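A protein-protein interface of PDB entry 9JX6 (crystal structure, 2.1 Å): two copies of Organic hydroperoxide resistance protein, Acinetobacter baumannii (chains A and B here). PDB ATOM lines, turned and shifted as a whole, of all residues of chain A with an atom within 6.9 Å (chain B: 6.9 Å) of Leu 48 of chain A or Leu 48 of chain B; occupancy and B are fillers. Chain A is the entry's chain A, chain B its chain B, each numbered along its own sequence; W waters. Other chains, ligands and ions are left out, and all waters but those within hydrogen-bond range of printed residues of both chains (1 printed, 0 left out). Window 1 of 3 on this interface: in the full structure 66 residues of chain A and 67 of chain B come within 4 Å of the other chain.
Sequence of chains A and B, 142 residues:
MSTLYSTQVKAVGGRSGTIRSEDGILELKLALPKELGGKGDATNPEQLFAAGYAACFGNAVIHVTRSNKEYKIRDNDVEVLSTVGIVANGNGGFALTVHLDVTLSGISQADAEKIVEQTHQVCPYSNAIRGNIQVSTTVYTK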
ATOM      1  N   THR A   7       3.625   2.470 -13.767  1.00  0.00           N
ATOM      2  CA  THR A   7       4.699   1.696 -13.166  1.00  0.00           C
ATOM      3  C   THR A   7       5.866   2.617 -12.847  1.00  0.00           C
ATOM      4  O   THR A   7       6.037   3.675 -13.455  1.00  0.00           O
ATOM      5  CB  THR A   7       5.159   0.548 -14.078  1.00  0.00           C
ATOM      6  OG1 THR A   7       5.985  -0.353 -13.333  1.00  0.00           O
ATOM      7  CG2 THR A   7       5.945   1.082 -15.269  1.00  0.00           C
ATOM      8  N   VAL A   9      10.174   2.615 -11.901  1.00  0.00           N
ATOM      9  CA  VAL A   9      11.452   1.915 -11.913  1.00  0.00           C
ATOM     10  C   VAL A   9      12.516   2.856 -11.371  1.00  0.00           C
ATOM     11  O   VAL A   9      12.601   4.016 -11.794  1.00  0.00           O
ATOM     12  CB  VAL A   9      11.837   1.427 -13.323  1.00  0.00           C
ATOM     13  CG1 VAL A   9      13.180   0.716 -13.278  1.00  0.00           C
ATOM     14  CG2 VAL A   9      10.764   0.506 -13.888  1.00  0.00           C
ATOM     15  N   ILE A  19      18.832  -1.331 -12.189  1.00  0.00           N
ATOM     16  CA  ILE A  19      17.435  -0.934 -12.301  1.00  0.00           C
ATOM     17  C   ILE A  19      16.611  -1.886 -11.449  1.00  0.00           C
ATOM     18  O   ILE A  19      16.929  -3.076 -11.346  1.00  0.00           O
ATOM     19  CB  ILE A  19      16.939  -0.951 -13.761  1.00  0.00           C
ATOM     20  CG1 ILE A  19      17.167  -2.337 -14.372  1.00  0.00           C
ATOM     21  CG2 ILE A  19      17.607   0.163 -14.573  1.00  0.00           C
ATOM     22  CD1 ILE A  19      16.120  -2.758 -15.364  1.00  0.00           C
ATOM     23  N   LEU A  26      10.915  -6.389 -12.136  1.00  0.00           N
ATOM     24  CA  LEU A  26      12.037  -6.140 -13.037  1.00  0.00           C
ATOM     25  C   LEU A  26      13.228  -5.661 -12.215  1.00  0.00           C
ATOM     26  O   LEU A  26      13.199  -4.561 -11.652  1.00  0.00           O
ATOM     27  CB  LEU A  26      11.660  -5.113 -14.103  1.00  0.00           C
ATOM     28  CG  LEU A  26      12.686  -4.870 -15.212  1.00  0.00           C
ATOM     29  CD1 LEU A  26      12.911  -6.137 -16.024  1.00  0.00           C
ATOM     30  CD2 LEU A  26      12.257  -3.711 -16.108  1.00  0.00           C
ATOM     31  N   LEU A  28      17.483  -5.740 -12.740  1.00  0.00           N
ATOM     32  CA  LEU A  28      18.534  -6.101 -13.679  1.00  0.00           C
ATOM     33  C   LEU A  28      19.793  -5.285 -13.426  1.00  0.00           C
ATOM     34  O   LEU A  28      19.732  -4.120 -13.025  1.00  0.00           O
ATOM     35  CB  LEU A  28      18.081  -5.892 -15.132  1.00  0.00           C
ATOM     36  CG  LEU A  28      16.965  -6.793 -15.667  1.00  0.00           C
ATOM     37  CD1 LEU A  28      16.707  -6.493 -17.131  1.00  0.00           C
ATOM     38  CD2 LEU A  28      17.319  -8.261 -15.479  1.00  0.00           C
ATOM     39  N   LEU A  30      23.165  -3.536 -15.201  1.00  0.00           N
ATOM     40  CA  LEU A  30      23.416  -2.844 -16.454  1.00  0.00           C
ATOM     41  C   LEU A  30      24.912  -2.736 -16.687  1.00  0.00           C
ATOM     42  O   LEU A  30      25.695  -2.579 -15.746  1.00  0.00           O
ATOM     43  CB  LEU A  30      22.797  -1.445 -16.459  1.00  0.00           C
ATOM     44  CG  LEU A  30      21.441  -1.281 -17.139  1.00  0.00           C
ATOM     45  CD1 LEU A  30      20.393  -2.211 -16.556  1.00  0.00           C
ATOM     46  CD2 LEU A  30      21.007   0.152 -17.013  1.00  0.00           C
ATOM     47  N   THR A  43      22.483  -5.942 -19.660  1.00  0.00           N
ATOM     48  CA  THR A  43      21.711  -5.208 -20.652  1.00  0.00           C
ATOM     49  C   THR A  43      22.048  -3.718 -20.581  1.00  0.00           C
ATOM     50  O   THR A  43      22.958  -3.292 -19.864  1.00  0.00           O
ATOM     51  CB  THR A  43      20.219  -5.480 -20.461  1.00  0.00           C
ATOM     52  OG1 THR A  43      19.485  -4.950 -21.570  1.00  0.00           O
ATOM     53  CG2 THR A  43      19.715  -4.856 -19.168  1.00  0.00           C
ATOM     54  N   ASN A  44      21.316  -2.907 -21.340  1.00  0.00           N
ATOM     55  CA  ASN A  44      21.614  -1.490 -21.477  1.00  0.00           C
ATOM     56  C   ASN A  44      20.340  -0.774 -21.911  1.00  0.00           C
ATOM     57  O   ASN A  44      19.377  -1.422 -22.343  1.00  0.00           O
ATOM     58  CB  ASN A  44      22.754  -1.265 -22.484  1.00  0.00           C
ATOM     59  CG  ASN A  44      22.468  -1.873 -23.838  1.00  0.00           C
ATOM     60  OD1 ASN A  44      21.523  -1.479 -24.523  1.00  0.00           O
ATOM     61  ND2 ASN A  44      23.281  -2.849 -24.230  1.00  0.00           N
ATOM     62  N   PRO A  45      20.295   0.561 -21.797  1.00  0.00           N
ATOM     63  CA  PRO A  45      19.049   1.277 -22.126  1.00  0.00           C
ATOM     64  C   PRO A  45      18.544   1.034 -23.539  1.00  0.00           C
ATOM     65  O   PRO A  45      17.327   1.058 -23.762  1.00  0.00           O
ATOM     66  CB  PRO A  45      19.435   2.746 -21.917  1.00  0.00           C
ATOM     67  CG  PRO A  45      20.483   2.688 -20.863  1.00  0.00           C
ATOM     68  CD  PRO A  45      21.294   1.467 -21.199  1.00  0.00           C
ATOM     69  N   GLU A  46      19.438   0.801 -24.502  1.00  0.00           N
ATOM     70  CA  GLU A  46      18.996   0.596 -25.877  1.00  0.00           C
ATOM     71  C   GLU A  46      18.291  -0.744 -26.036  1.00  0.00           C
ATOM     72  O   GLU A  46      17.292  -0.843 -26.755  1.00  0.00           O
ATOM     73  CB  GLU A  46      20.186   0.705 -26.829  1.00  0.00           C
ATOM     74  CG  GLU A  46      20.659   2.136 -27.071  1.00  0.00           C
ATOM     75  CD  GLU A  46      21.259   2.778 -25.828  1.00  0.00           C
ATOM     76  OE1 GLU A  46      22.080   2.124 -25.149  1.00  0.00           O
ATOM     77  OE2 GLU A  46      20.900   3.935 -25.524  1.00  0.00           O
ATOM     78  N   GLN A  47      18.797  -1.785 -25.367  1.00  0.00           N
ATOM     79  CA  GLN A  47      18.127  -3.080 -25.397  1.00  0.00           C
ATOM     80  C   GLN A  47      16.767  -3.010 -24.715  1.00  0.00           C
ATOM     81  O   GLN A  47      15.788  -3.577 -25.212  1.00  0.00           O
ATOM     82  CB  GLN A  47      19.001  -4.141 -24.729  1.00  0.00           C
ATOM     83  CG  GLN A  47      20.164  -4.606 -25.580  1.00  0.00           C
ATOM     84  CD  GLN A  47      20.784  -5.892 -25.072  1.00  0.00           C
ATOM     85  OE1 GLN A  47      20.630  -6.250 -23.905  1.00  0.00           O
ATOM     86  NE2 GLN A  47      21.493  -6.594 -25.949  1.00  0.00           N
ATOM     87  N   LEU A  48      16.692  -2.320 -23.575  1.00  0.00           N
ATOM     88  CA  LEU A  48      15.419  -2.174 -22.877  1.00  0.00           C
ATOM     89  C   LEU A  48      14.397  -1.450 -23.743  1.00  0.00           C
ATOM     90  O   LEU A  48      13.227  -1.847 -23.796  1.00  0.00           O
ATOM     91  CB  LEU A  48      15.634  -1.432 -21.557  1.00  0.00           C
ATOM     92  CG  LEU A  48      16.412  -2.214 -20.497  1.00  0.00           C
ATOM     93  CD1 LEU A  48      16.871  -1.304 -19.366  1.00  0.00           C
ATOM     94  CD2 LEU A  48      15.571  -3.356 -19.956  1.00  0.00           C
ATOM     95  N   PHE A  49      14.820  -0.391 -24.438  1.00  0.00           N
ATOM     96  CA  PHE A  49      13.900   0.318 -25.322  1.00  0.00           C
ATOM     97  C   PHE A  49      13.497  -0.545 -26.509  1.00  0.00           C
ATOM     98  O   PHE A  49      12.317  -0.591 -26.874  1.00  0.00           O
ATOM     99  CB  PHE A  49      14.524   1.624 -25.809  1.00  0.00           C
ATOM    100  CG  PHE A  49      13.605   2.438 -26.673  1.00  0.00           C
ATOM    101  CD1 PHE A  49      12.572   3.168 -26.111  1.00  0.00           C
ATOM    102  CD2 PHE A  49      13.759   2.452 -28.050  1.00  0.00           C
ATOM    103  CE1 PHE A  49      11.717   3.910 -26.904  1.00  0.00           C
ATOM    104  CE2 PHE A  49      12.908   3.194 -28.848  1.00  0.00           C
ATOM    105  CZ  PHE A  49      11.885   3.923 -28.274  1.00  0.00           C
ATOM    106  N   ALA A  50      14.463  -1.231 -27.129  1.00  0.00           N
ATOM    107  CA  ALA A  50      14.136  -2.115 -28.243  1.00  0.00           C
ATOM    108  C   ALA A  50      13.139  -3.185 -27.816  1.00  0.00           C
ATOM    109  O   ALA A  50      12.229  -3.534 -28.577  1.00  0.00           O
ATOM    110  CB  ALA A  50      15.410  -2.757 -28.797  1.00  0.00           C
ATOM    111  N   ALA A  51      13.283  -3.698 -26.593  1.00  0.00           N
ATOM    112  CA  ALA A  51      12.391  -4.748 -26.111  1.00  0.00           C
ATOM    113  C   ALA A  51      10.988  -4.209 -25.861  1.00  0.00           C
ATOM    114  O   ALA A  51       9.994  -4.831 -26.255  1.00  0.00           O
ATOM    115  CB  ALA A  51      12.963  -5.374 -24.839  1.00  0.00           C
ATOM    116  N   GLY A  52      10.889  -3.057 -25.197  1.00  0.00           N
ATOM    117  CA  GLY A  52       9.583  -2.471 -24.949  1.00  0.00           C
ATOM    118  C   GLY A  52       8.863  -2.097 -26.230  1.00  0.00           C
ATOM    119  O   GLY A  52       7.679  -2.399 -26.403  1.00  0.00           O
ATOM    120  N   TYR A  53       9.575  -1.435 -27.147  1.00  0.00           N
ATOM    121  CA  TYR A  53       8.978  -1.034 -28.419  1.00  0.00           C
ATOM    122  C   TYR A  53       8.494  -2.246 -29.205  1.00  0.00           C
ATOM    123  O   TYR A  53       7.341  -2.293 -29.650  1.00  0.00           O
ATOM    124  CB  TYR A  53       9.993  -0.231 -29.236  1.00  0.00           C
ATOM    125  CG  TYR A  53       9.410   0.588 -30.376  1.00  0.00           C
ATOM    126  CD1 TYR A  53       8.065   0.500 -30.720  1.00  0.00           C
ATOM    127  CD2 TYR A  53      10.213   1.458 -31.104  1.00  0.00           C
ATOM    128  CE1 TYR A  53       7.539   1.247 -31.761  1.00  0.00           C
ATOM    129  CE2 TYR A  53       9.696   2.211 -32.143  1.00  0.00           C
ATOM    130  CZ  TYR A  53       8.360   2.101 -32.468  1.00  0.00           C
ATOM    131  OH  TYR A  53       7.845   2.851 -33.501  1.00  0.00           O
ATOM    132  N   ALA A  55       7.679  -5.102 -28.233  1.00  0.00           N
ATOM    133  CA  ALA A  55       6.569  -5.779 -27.573  1.00  0.00           C
ATOM    134  C   ALA A  55       5.258  -5.013 -27.725  1.00  0.00           C
ATOM    135  O   ALA A  55       4.208  -5.627 -27.942  1.00  0.00           O
ATOM    136  CB  ALA A  55       6.898  -5.997 -26.100  1.00  0.00           C
ATOM    137  N   TYR A 125       4.423   3.896 -28.445  1.00  0.00           N
ATOM    138  CA  TYR A 125       5.841   4.190 -28.633  1.00  0.00           C
ATOM    139  C   TYR A 125       6.103   4.843 -29.980  1.00  0.00           C
ATOM    140  O   TYR A 125       6.938   5.748 -30.079  1.00  0.00           O
ATOM    141  CB  TYR A 125       6.657   2.909 -28.470  1.00  0.00           C
ATOM    142  CG  TYR A 125       6.565   2.383 -27.062  1.00  0.00           C
ATOM    143  CD1 TYR A 125       5.527   1.554 -26.689  1.00  0.00           C
ATOM    144  CD2 TYR A 125       7.508   2.721 -26.106  1.00  0.00           C
ATOM    145  CE1 TYR A 125       5.416   1.077 -25.408  1.00  0.00           C
ATOM    146  CE2 TYR A 125       7.410   2.242 -24.813  1.00  0.00           C
ATOM    147  CZ  TYR A 125       6.359   1.418 -24.473  1.00  0.00           C
ATOM    148  OH  TYR A 125       6.247   0.935 -23.194  1.00  0.00           O
ATOM    149  N   THR B   7      21.771  -2.567 -31.272  1.00  0.00           N
ATOM    150  CA  THR B   7      21.364  -3.834 -30.685  1.00  0.00           C
ATOM    151  C   THR B   7      20.015  -4.237 -31.259  1.00  0.00           C
ATOM    152  O   THR B   7      19.240  -3.400 -31.727  1.00  0.00           O
ATOM    153  CB  THR B   7      21.301  -3.749 -29.155  1.00  0.00           C
ATOM    154  OG1 THR B   7      21.051  -5.051 -28.612  1.00  0.00           O
ATOM    155  CG2 THR B   7      20.201  -2.785 -28.714  1.00  0.00           C
ATOM    156  N   VAL B   9      16.478  -6.734 -30.628  1.00  0.00           N
ATOM    157  CA  VAL B   9      15.636  -7.483 -29.704  1.00  0.00           C
ATOM    158  C   VAL B   9      14.438  -8.036 -30.464  1.00  0.00           C
ATOM    159  O   VAL B   9      13.818  -7.331 -31.269  1.00  0.00           O
ATOM    160  CB  VAL B   9      15.172  -6.619 -28.514  1.00  0.00           C
ATOM    161  CG1 VAL B   9      14.256  -7.435 -27.602  1.00  0.00           C
ATOM    162  CG2 VAL B   9      16.368  -6.112 -27.733  1.00  0.00           C
ATOM    163  N   ILE B  19      10.452 -11.663 -25.004  1.00  0.00           N
ATOM    164  CA  ILE B  19      11.439 -10.801 -25.644  1.00  0.00           C
ATOM    165  C   ILE B  19      12.812 -11.417 -25.429  1.00  0.00           C
ATOM    166  O   ILE B  19      13.082 -12.005 -24.376  1.00  0.00           O
ATOM    167  CB  ILE B  19      11.393  -9.360 -25.097  1.00  0.00           C
ATOM    168  CG1 ILE B  19      11.458  -9.372 -23.572  1.00  0.00           C
ATOM    169  CG2 ILE B  19      10.145  -8.638 -25.576  1.00  0.00           C
ATOM    170  CD1 ILE B  19      12.338  -8.303 -22.995  1.00  0.00           C
ATOM    171  N   LEU B  26      19.585 -10.097 -22.791  1.00  0.00           N
ATOM    172  CA  LEU B  26      18.262  -9.749 -22.292  1.00  0.00           C
ATOM    173  C   LEU B  26      17.260 -10.764 -22.820  1.00  0.00           C
ATOM    174  O   LEU B  26      17.071 -10.880 -24.035  1.00  0.00           O
ATOM    175  CB  LEU B  26      17.873  -8.331 -22.715  1.00  0.00           C
ATOM    176  CG  LEU B  26      16.589  -7.754 -22.113  1.00  0.00           C
ATOM    177  CD1 LEU B  26      16.750  -7.561 -20.620  1.00  0.00           C
ATOM    178  CD2 LEU B  26      16.232  -6.436 -22.782  1.00  0.00           C
ATOM    179  N   LEU B  28      13.412 -12.441 -21.324  1.00  0.00           N
ATOM    180  CA  LEU B  28      12.431 -12.603 -20.260  1.00  0.00           C
ATOM    181  C   LEU B  28      11.031 -12.608 -20.855  1.00  0.00           C
ATOM    182  O   LEU B  28      10.809 -12.165 -21.985  1.00  0.00           O
ATOM    183  CB  LEU B  28      12.564 -11.513 -19.184  1.00  0.00           C
ATOM    184  CG  LEU B  28      12.557 -10.020 -19.518  1.00  0.00           C
ATOM    185  CD1 LEU B  28      12.214  -9.242 -18.269  1.00  0.00           C
ATOM    186  CD2 LEU B  28      13.908  -9.568 -20.018  1.00  0.00           C
ATOM    187  N   LEU B  30       6.863 -11.674 -20.768  1.00  0.00           N
ATOM    188  CA  LEU B  30       6.011 -10.533 -20.483  1.00  0.00           C
ATOM    189  C   LEU B  30       4.632 -11.006 -20.052  1.00  0.00           C
ATOM    190  O   LEU B  30       4.176 -12.087 -20.436  1.00  0.00           O
ATOM    191  CB  LEU B  30       5.860  -9.617 -21.698  1.00  0.00           C
ATOM    192  CG  LEU B  30       7.102  -9.145 -22.450  1.00  0.00           C
ATOM    193  CD1 LEU B  30       6.712  -7.973 -23.304  1.00  0.00           C
ATOM    194  CD2 LEU B  30       8.221  -8.760 -21.507  1.00  0.00           C
ATOM    195  N   THR B  43       7.275  -8.661 -16.527  1.00  0.00           N
ATOM    196  CA  THR B  43       7.383  -7.254 -16.870  1.00  0.00           C
ATOM    197  C   THR B  43       6.505  -6.935 -18.082  1.00  0.00           C
ATOM    198  O   THR B  43       5.773  -7.784 -18.599  1.00  0.00           O
ATOM    199  CB  THR B  43       8.847  -6.888 -17.118  1.00  0.00           C
ATOM    200  OG1 THR B  43       9.015  -5.472 -16.999  1.00  0.00           O
ATOM    201  CG2 THR B  43       9.290  -7.338 -18.497  1.00  0.00           C
ATOM    202  N   ASN B  44       6.577  -5.689 -18.530  1.00  0.00           N
ATOM    203  CA  ASN B  44       5.708  -5.184 -19.581  1.00  0.00           C
ATOM    204  C   ASN B  44       6.435  -4.069 -20.302  1.00  0.00           C
ATOM    205  O   ASN B  44       7.467  -3.570 -19.817  1.00  0.00           O
ATOM    206  CB  ASN B  44       4.373  -4.694 -19.002  1.00  0.00           C
ATOM    207  CG  ASN B  44       4.560  -3.713 -17.863  1.00  0.00           C
ATOM    208  OD1 ASN B  44       5.118  -2.630 -18.043  1.00  0.00           O
ATOM    209  ND2 ASN B  44       4.094  -4.090 -16.677  1.00  0.00           N
ATOM    210  N   PRO B  45       5.953  -3.653 -21.482  1.00  0.00           N
ATOM    211  CA  PRO B  45       6.642  -2.580 -22.217  1.00  0.00           C
ATOM    212  C   PRO B  45       6.829  -1.301 -21.416  1.00  0.00           C
ATOM    213  O   PRO B  45       7.885  -0.664 -21.521  1.00  0.00           O
ATOM    214  CB  PRO B  45       5.732  -2.361 -23.431  1.00  0.00           C
ATOM    215  CG  PRO B  45       5.137  -3.705 -23.670  1.00  0.00           C
ATOM    216  CD  PRO B  45       4.867  -4.246 -22.291  1.00  0.00           C
ATOM    217  N   GLU B  46       5.835  -0.902 -20.619  1.00  0.00           N
ATOM    218  CA  GLU B  46       5.959   0.335 -19.855  1.00  0.00           C
ATOM    219  C   GLU B  46       7.073   0.228 -18.827  1.00  0.00           C
ATOM    220  O   GLU B  46       7.841   1.176 -18.624  1.00  0.00           O
ATOM    221  CB  GLU B  46       4.634   0.675 -19.175  1.00  0.00           C
ATOM    222  CG  GLU B  46       3.582   1.235 -20.117  1.00  0.00           C
ATOM    223  CD  GLU B  46       3.133   0.224 -21.153  1.00  0.00           C
ATOM    224  OE1 GLU B  46       2.668  -0.867 -20.758  1.00  0.00           O
ATOM    225  OE2 GLU B  46       3.259   0.512 -22.360  1.00  0.00           O
ATOM    226  N   GLN B  47       7.180  -0.931 -18.179  1.00  0.00           N
ATOM    227  CA  GLN B  47       8.248  -1.167 -17.215  1.00  0.00           C
ATOM    228  C   GLN B  47       9.615  -1.157 -17.889  1.00  0.00           C
ATOM    229  O   GLN B  47      10.585  -0.633 -17.330  1.00  0.00           O
ATOM    230  CB  GLN B  47       7.996  -2.499 -16.510  1.00  0.00           C
ATOM    231  CG  GLN B  47       8.239  -2.513 -15.024  1.00  0.00           C
ATOM    232  CD  GLN B  47       7.724  -3.788 -14.381  1.00  0.00           C
ATOM    233  OE1 GLN B  47       8.313  -4.855 -14.534  1.00  0.00           O
ATOM    234  NE2 GLN B  47       6.618  -3.678 -13.652  1.00  0.00           N
ATOM    235  N   LEU B  48       9.708  -1.734 -19.090  1.00  0.00           N
ATOM    236  CA  LEU B  48      10.975  -1.752 -19.815  1.00  0.00           C
ATOM    237  C   LEU B  48      11.373  -0.349 -20.262  1.00  0.00           C
ATOM    238  O   LEU B  48      12.542   0.041 -20.141  1.00  0.00           O
ATOM    239  CB  LEU B  48      10.873  -2.695 -21.015  1.00  0.00           C
ATOM    240  CG  LEU B  48      10.782  -4.192 -20.694  1.00  0.00           C
ATOM    241  CD1 LEU B  48      10.256  -4.975 -21.892  1.00  0.00           C
ATOM    242  CD2 LEU B  48      12.129  -4.737 -20.242  1.00  0.00           C
ATOM    243  N   PHE B  49      10.414   0.423 -20.783  1.00  0.00           N
ATOM    244  CA  PHE B  49      10.682   1.815 -21.135  1.00  0.00           C
ATOM    245  C   PHE B  49      11.102   2.619 -19.908  1.00  0.00           C
ATOM    246  O   PHE B  49      12.084   3.370 -19.950  1.00  0.00           O
ATOM    247  CB  PHE B  49       9.441   2.430 -21.784  1.00  0.00           C
ATOM    248  CG  PHE B  49       9.621   3.856 -22.219  1.00  0.00           C
ATOM    249  CD1 PHE B  49      10.533   4.182 -23.208  1.00  0.00           C
ATOM    250  CD2 PHE B  49       8.876   4.868 -21.641  1.00  0.00           C
ATOM    251  CE1 PHE B  49      10.698   5.495 -23.612  1.00  0.00           C
ATOM    252  CE2 PHE B  49       9.038   6.183 -22.041  1.00  0.00           C
ATOM    253  CZ  PHE B  49       9.950   6.495 -23.026  1.00  0.00           C
ATOM    254  N   ALA B  50      10.367   2.469 -18.802  1.00  0.00           N
ATOM    255  CA  ALA B  50      10.713   3.182 -17.573  1.00  0.00           C
ATOM    256  C   ALA B  50      12.139   2.884 -17.138  1.00  0.00           C
ATOM    257  O   ALA B  50      12.872   3.786 -16.715  1.00  0.00           O
ATOM    258  CB  ALA B  50       9.735   2.812 -16.459  1.00  0.00           C
ATOM    259  N   ALA B  51      12.552   1.620 -17.233  1.00  0.00           N
ATOM    260  CA  ALA B  51      13.888   1.241 -16.789  1.00  0.00           C
ATOM    261  C   ALA B  51      14.958   1.835 -17.697  1.00  0.00           C
ATOM    262  O   ALA B  51      15.956   2.385 -17.216  1.00  0.00           O
ATOM    263  CB  ALA B  51      14.002  -0.282 -16.734  1.00  0.00           C
ATOM    264  N   GLY B  52      14.769   1.733 -19.013  1.00  0.00           N
ATOM    265  CA  GLY B  52      15.757   2.269 -19.934  1.00  0.00           C
ATOM    266  C   GLY B  52      15.873   3.780 -19.853  1.00  0.00           C
ATOM    267  O   GLY B  52      16.976   4.331 -19.917  1.00  0.00           O
ATOM    268  N   TYR B  53      14.740   4.469 -19.706  1.00  0.00           N
ATOM    269  CA  TYR B  53      14.767   5.922 -19.575  1.00  0.00           C
ATOM    270  C   TYR B  53      15.483   6.338 -18.297  1.00  0.00           C
ATOM    271  O   TYR B  53      16.405   7.161 -18.328  1.00  0.00           O
ATOM    272  CB  TYR B  53      13.339   6.473 -19.603  1.00  0.00           C
ATOM    273  CG  TYR B  53      13.218   7.956 -19.909  1.00  0.00           C
ATOM    274  CD1 TYR B  53      14.337   8.783 -19.953  1.00  0.00           C
ATOM    275  CD2 TYR B  53      11.980   8.526 -20.157  1.00  0.00           C
ATOM    276  CE1 TYR B  53      14.219  10.133 -20.230  1.00  0.00           C
ATOM    277  CE2 TYR B  53      11.853   9.873 -20.436  1.00  0.00           C
ATOM    278  CZ  TYR B  53      12.973  10.671 -20.472  1.00  0.00           C
ATOM    279  OH  TYR B  53      12.838  12.010 -20.752  1.00  0.00           O
ATOM    280  N   ALA B  55      17.635   4.864 -16.591  1.00  0.00           N
ATOM    281  CA  ALA B  55      19.059   4.557 -16.640  1.00  0.00           C
ATOM    282  C   ALA B  55      19.808   5.471 -17.607  1.00  0.00           C
ATOM    283  O   ALA B  55      20.915   5.923 -17.292  1.00  0.00           O
ATOM    284  CB  ALA B  55      19.258   3.091 -17.019  1.00  0.00           C
ATOM    285  N   TYR B 125      16.657   9.521 -24.904  1.00  0.00           N
ATOM    286  CA  TYR B 125      15.247   9.272 -24.611  1.00  0.00           C
ATOM    287  C   TYR B 125      14.455  10.572 -24.597  1.00  0.00           C
ATOM    288  O   TYR B 125      13.380  10.662 -25.202  1.00  0.00           O
ATOM    289  CB  TYR B 125      15.094   8.566 -23.268  1.00  0.00           C
ATOM    290  CG  TYR B 125      15.287   7.074 -23.289  1.00  0.00           C
ATOM    291  CD1 TYR B 125      16.530   6.518 -23.542  1.00  0.00           C
ATOM    292  CD2 TYR B 125      14.225   6.219 -23.025  1.00  0.00           C
ATOM    293  CE1 TYR B 125      16.709   5.151 -23.540  1.00  0.00           C
ATOM    294  CE2 TYR B 125      14.393   4.850 -23.021  1.00  0.00           C
ATOM    295  CZ  TYR B 125      15.638   4.321 -23.283  1.00  0.00           C
ATOM    296  OH  TYR B 125      15.814   2.957 -23.282  1.00  0.00           O
HETATM  297  O   HOH W   1      18.375   3.662 -25.450  1.00  0.00           O
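OG1 of Thr 7 of chain B lies within hydrogen-bond range of NE2 of Gln 47 of chain A, 3.1 Å away.
The backbone carbonyl oxygen of Pro 45 of chain B sits at hydrogen-bond distance from the side-chain hydroxyl of Tyr 125 of chain A.
OE2 of Glu 46 of chain B sits at hydrogen-bond distance from OH of Tyr 125 of chain A, 3.1 Å away.
NE2 of Gln 47 of chain B is in hydrogen-bond range of OG1 of Thr 7 of chain A.
The side-chain hydroxyl (OH) of Tyr 125 of chain B is in hydrogen-bond range of the backbone carbonyl oxygen (O) of Pro 45 of chain A (2.5 Å).
OE1 of Gln 47 of chain B sits at hydrogen-bond distance from OG1 of Thr 43 of chain B (2.6 Å).
The backbone NH (N) of Glu 46 of chain B sits at hydrogen-bond distance from the side-chain amide oxygen (OD1) of Asn 44 of chain B.
N of Ile 19 of chain A is in hydrogen-bond range of O of Leu 28 of chain A (3.0 Å).
OG1 of Thr 43 of chain A lies within hydrogen-bond range of OE1 of Gln 47 of chain A.
The side-chain amide oxygen (OD1) of Asn 44 of chain A lies within hydrogen-bond range of the backbone NH (N) of Gln 47 of chain A, at 2.9 Å.
CG2 of Val 9 of chain A touches CB of Ala 50 of chain B (3.6 Å).
Ile 19 of chain A touches Ala 51 of chain B.
CD2 of Leu 26 of chain A touches OG1 of Thr 43 of chain B, 3.8 Å away.
CD1 of Leu 28 of chain A touches CD1 of Leu 26 of chain B, at 3.6 Å.
Ala 55 of chain B touches Leu 30 of chain A.
Thr 43 of chain A touches Leu 26 of chain B.
CB of Pro 45 of chain A touches O of Gly 52 of chain B, 3.5 Å away.
CB of Phe 49 of chain A touches OH of Tyr 125 of chain B (3.1 Å).
Ile 19 of chain B touches Ala 51 of chain A.
Of chain B, only Leu 48 and Gly 52 come within 4 Å of Leu 48 of chain A.
Leu 48 of chain B touches just these residues of chain A: Leu 48 and Gly 52.
Of the printed residues of chain A, Ile 19 of chain B touches Ala 51 (3.5 Å).
Of the printed residues of chain A, Glu 46 of chain B touches Thr 7 and Tyr 125.
Asn 44 of chain B touches none of the printed residues of chain A.
Tyr 53 of chain B touches none of the printed residues of chain A.
The nearest residue of chain A that does not touch Leu 48 of chain B is Ala 51 of chain A (4.02 Å).
The nearest printed residue of chain A that does not touch Leu 30 of chain B is Ala 51 of chain A (5.4 Å).
Printed residues of chain B that touch a printed residue of chain A: Thr 7, Val 9, Ile 19, Leu 26, Leu 28, Leu 30, Thr 43, Pro 45, Glu 46, Gln 47, Leu 48, Phe 49, Ala 50, Ala 51, Gly 52, Ala 55 and Tyr 125.
Hydrophobic or aromatic side chains of chain B that line the printed part of chain A: Val 9, Ile 19, Leu 26, Leu 28, Leu 30, Pro 45, Leu 48, Phe 49, Ala 50, Ala 51, Ala 55 and Tyr 125.
Hydrophobic or aromatic side chains of chain A within 4 Å of the printed part of chain B: Val 9, Ile 19, Leu 26, Leu 28, Leu 30, Pro 45, Leu 48, Phe 49, Ala 50, Ala 51, Ala 55 and Tyr 125.
Val 9 of chain A touches Gln 47 of chain B, and with the chains exchanged Gln 47 of chain A touches Val 9 of chain B.
Leu 30 of chain A touches Ala 55 of chain B, and with the chains exchanged Ala 55 of chain A touches Leu 30 of chain B.
Pro 45 of chain A touches Gly 52 of chain B, and with the chains exchanged Gly 52 of chain A touches Pro 45 of chain B.
Of the 33 pairs that touch across the chains among the printed residues, 30 have their exchanged pair printed and touching as well.
Water W1 lies within hydrogen-bond range of the side-chain carboxylate of Glu 46 of chain A (2.5 Å), the backbone carbonyl oxygen of Pro 45 of chain A (3.3 Å) and the side-chain hydroxyl of Tyr 125 of chain B (3.4 Å).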
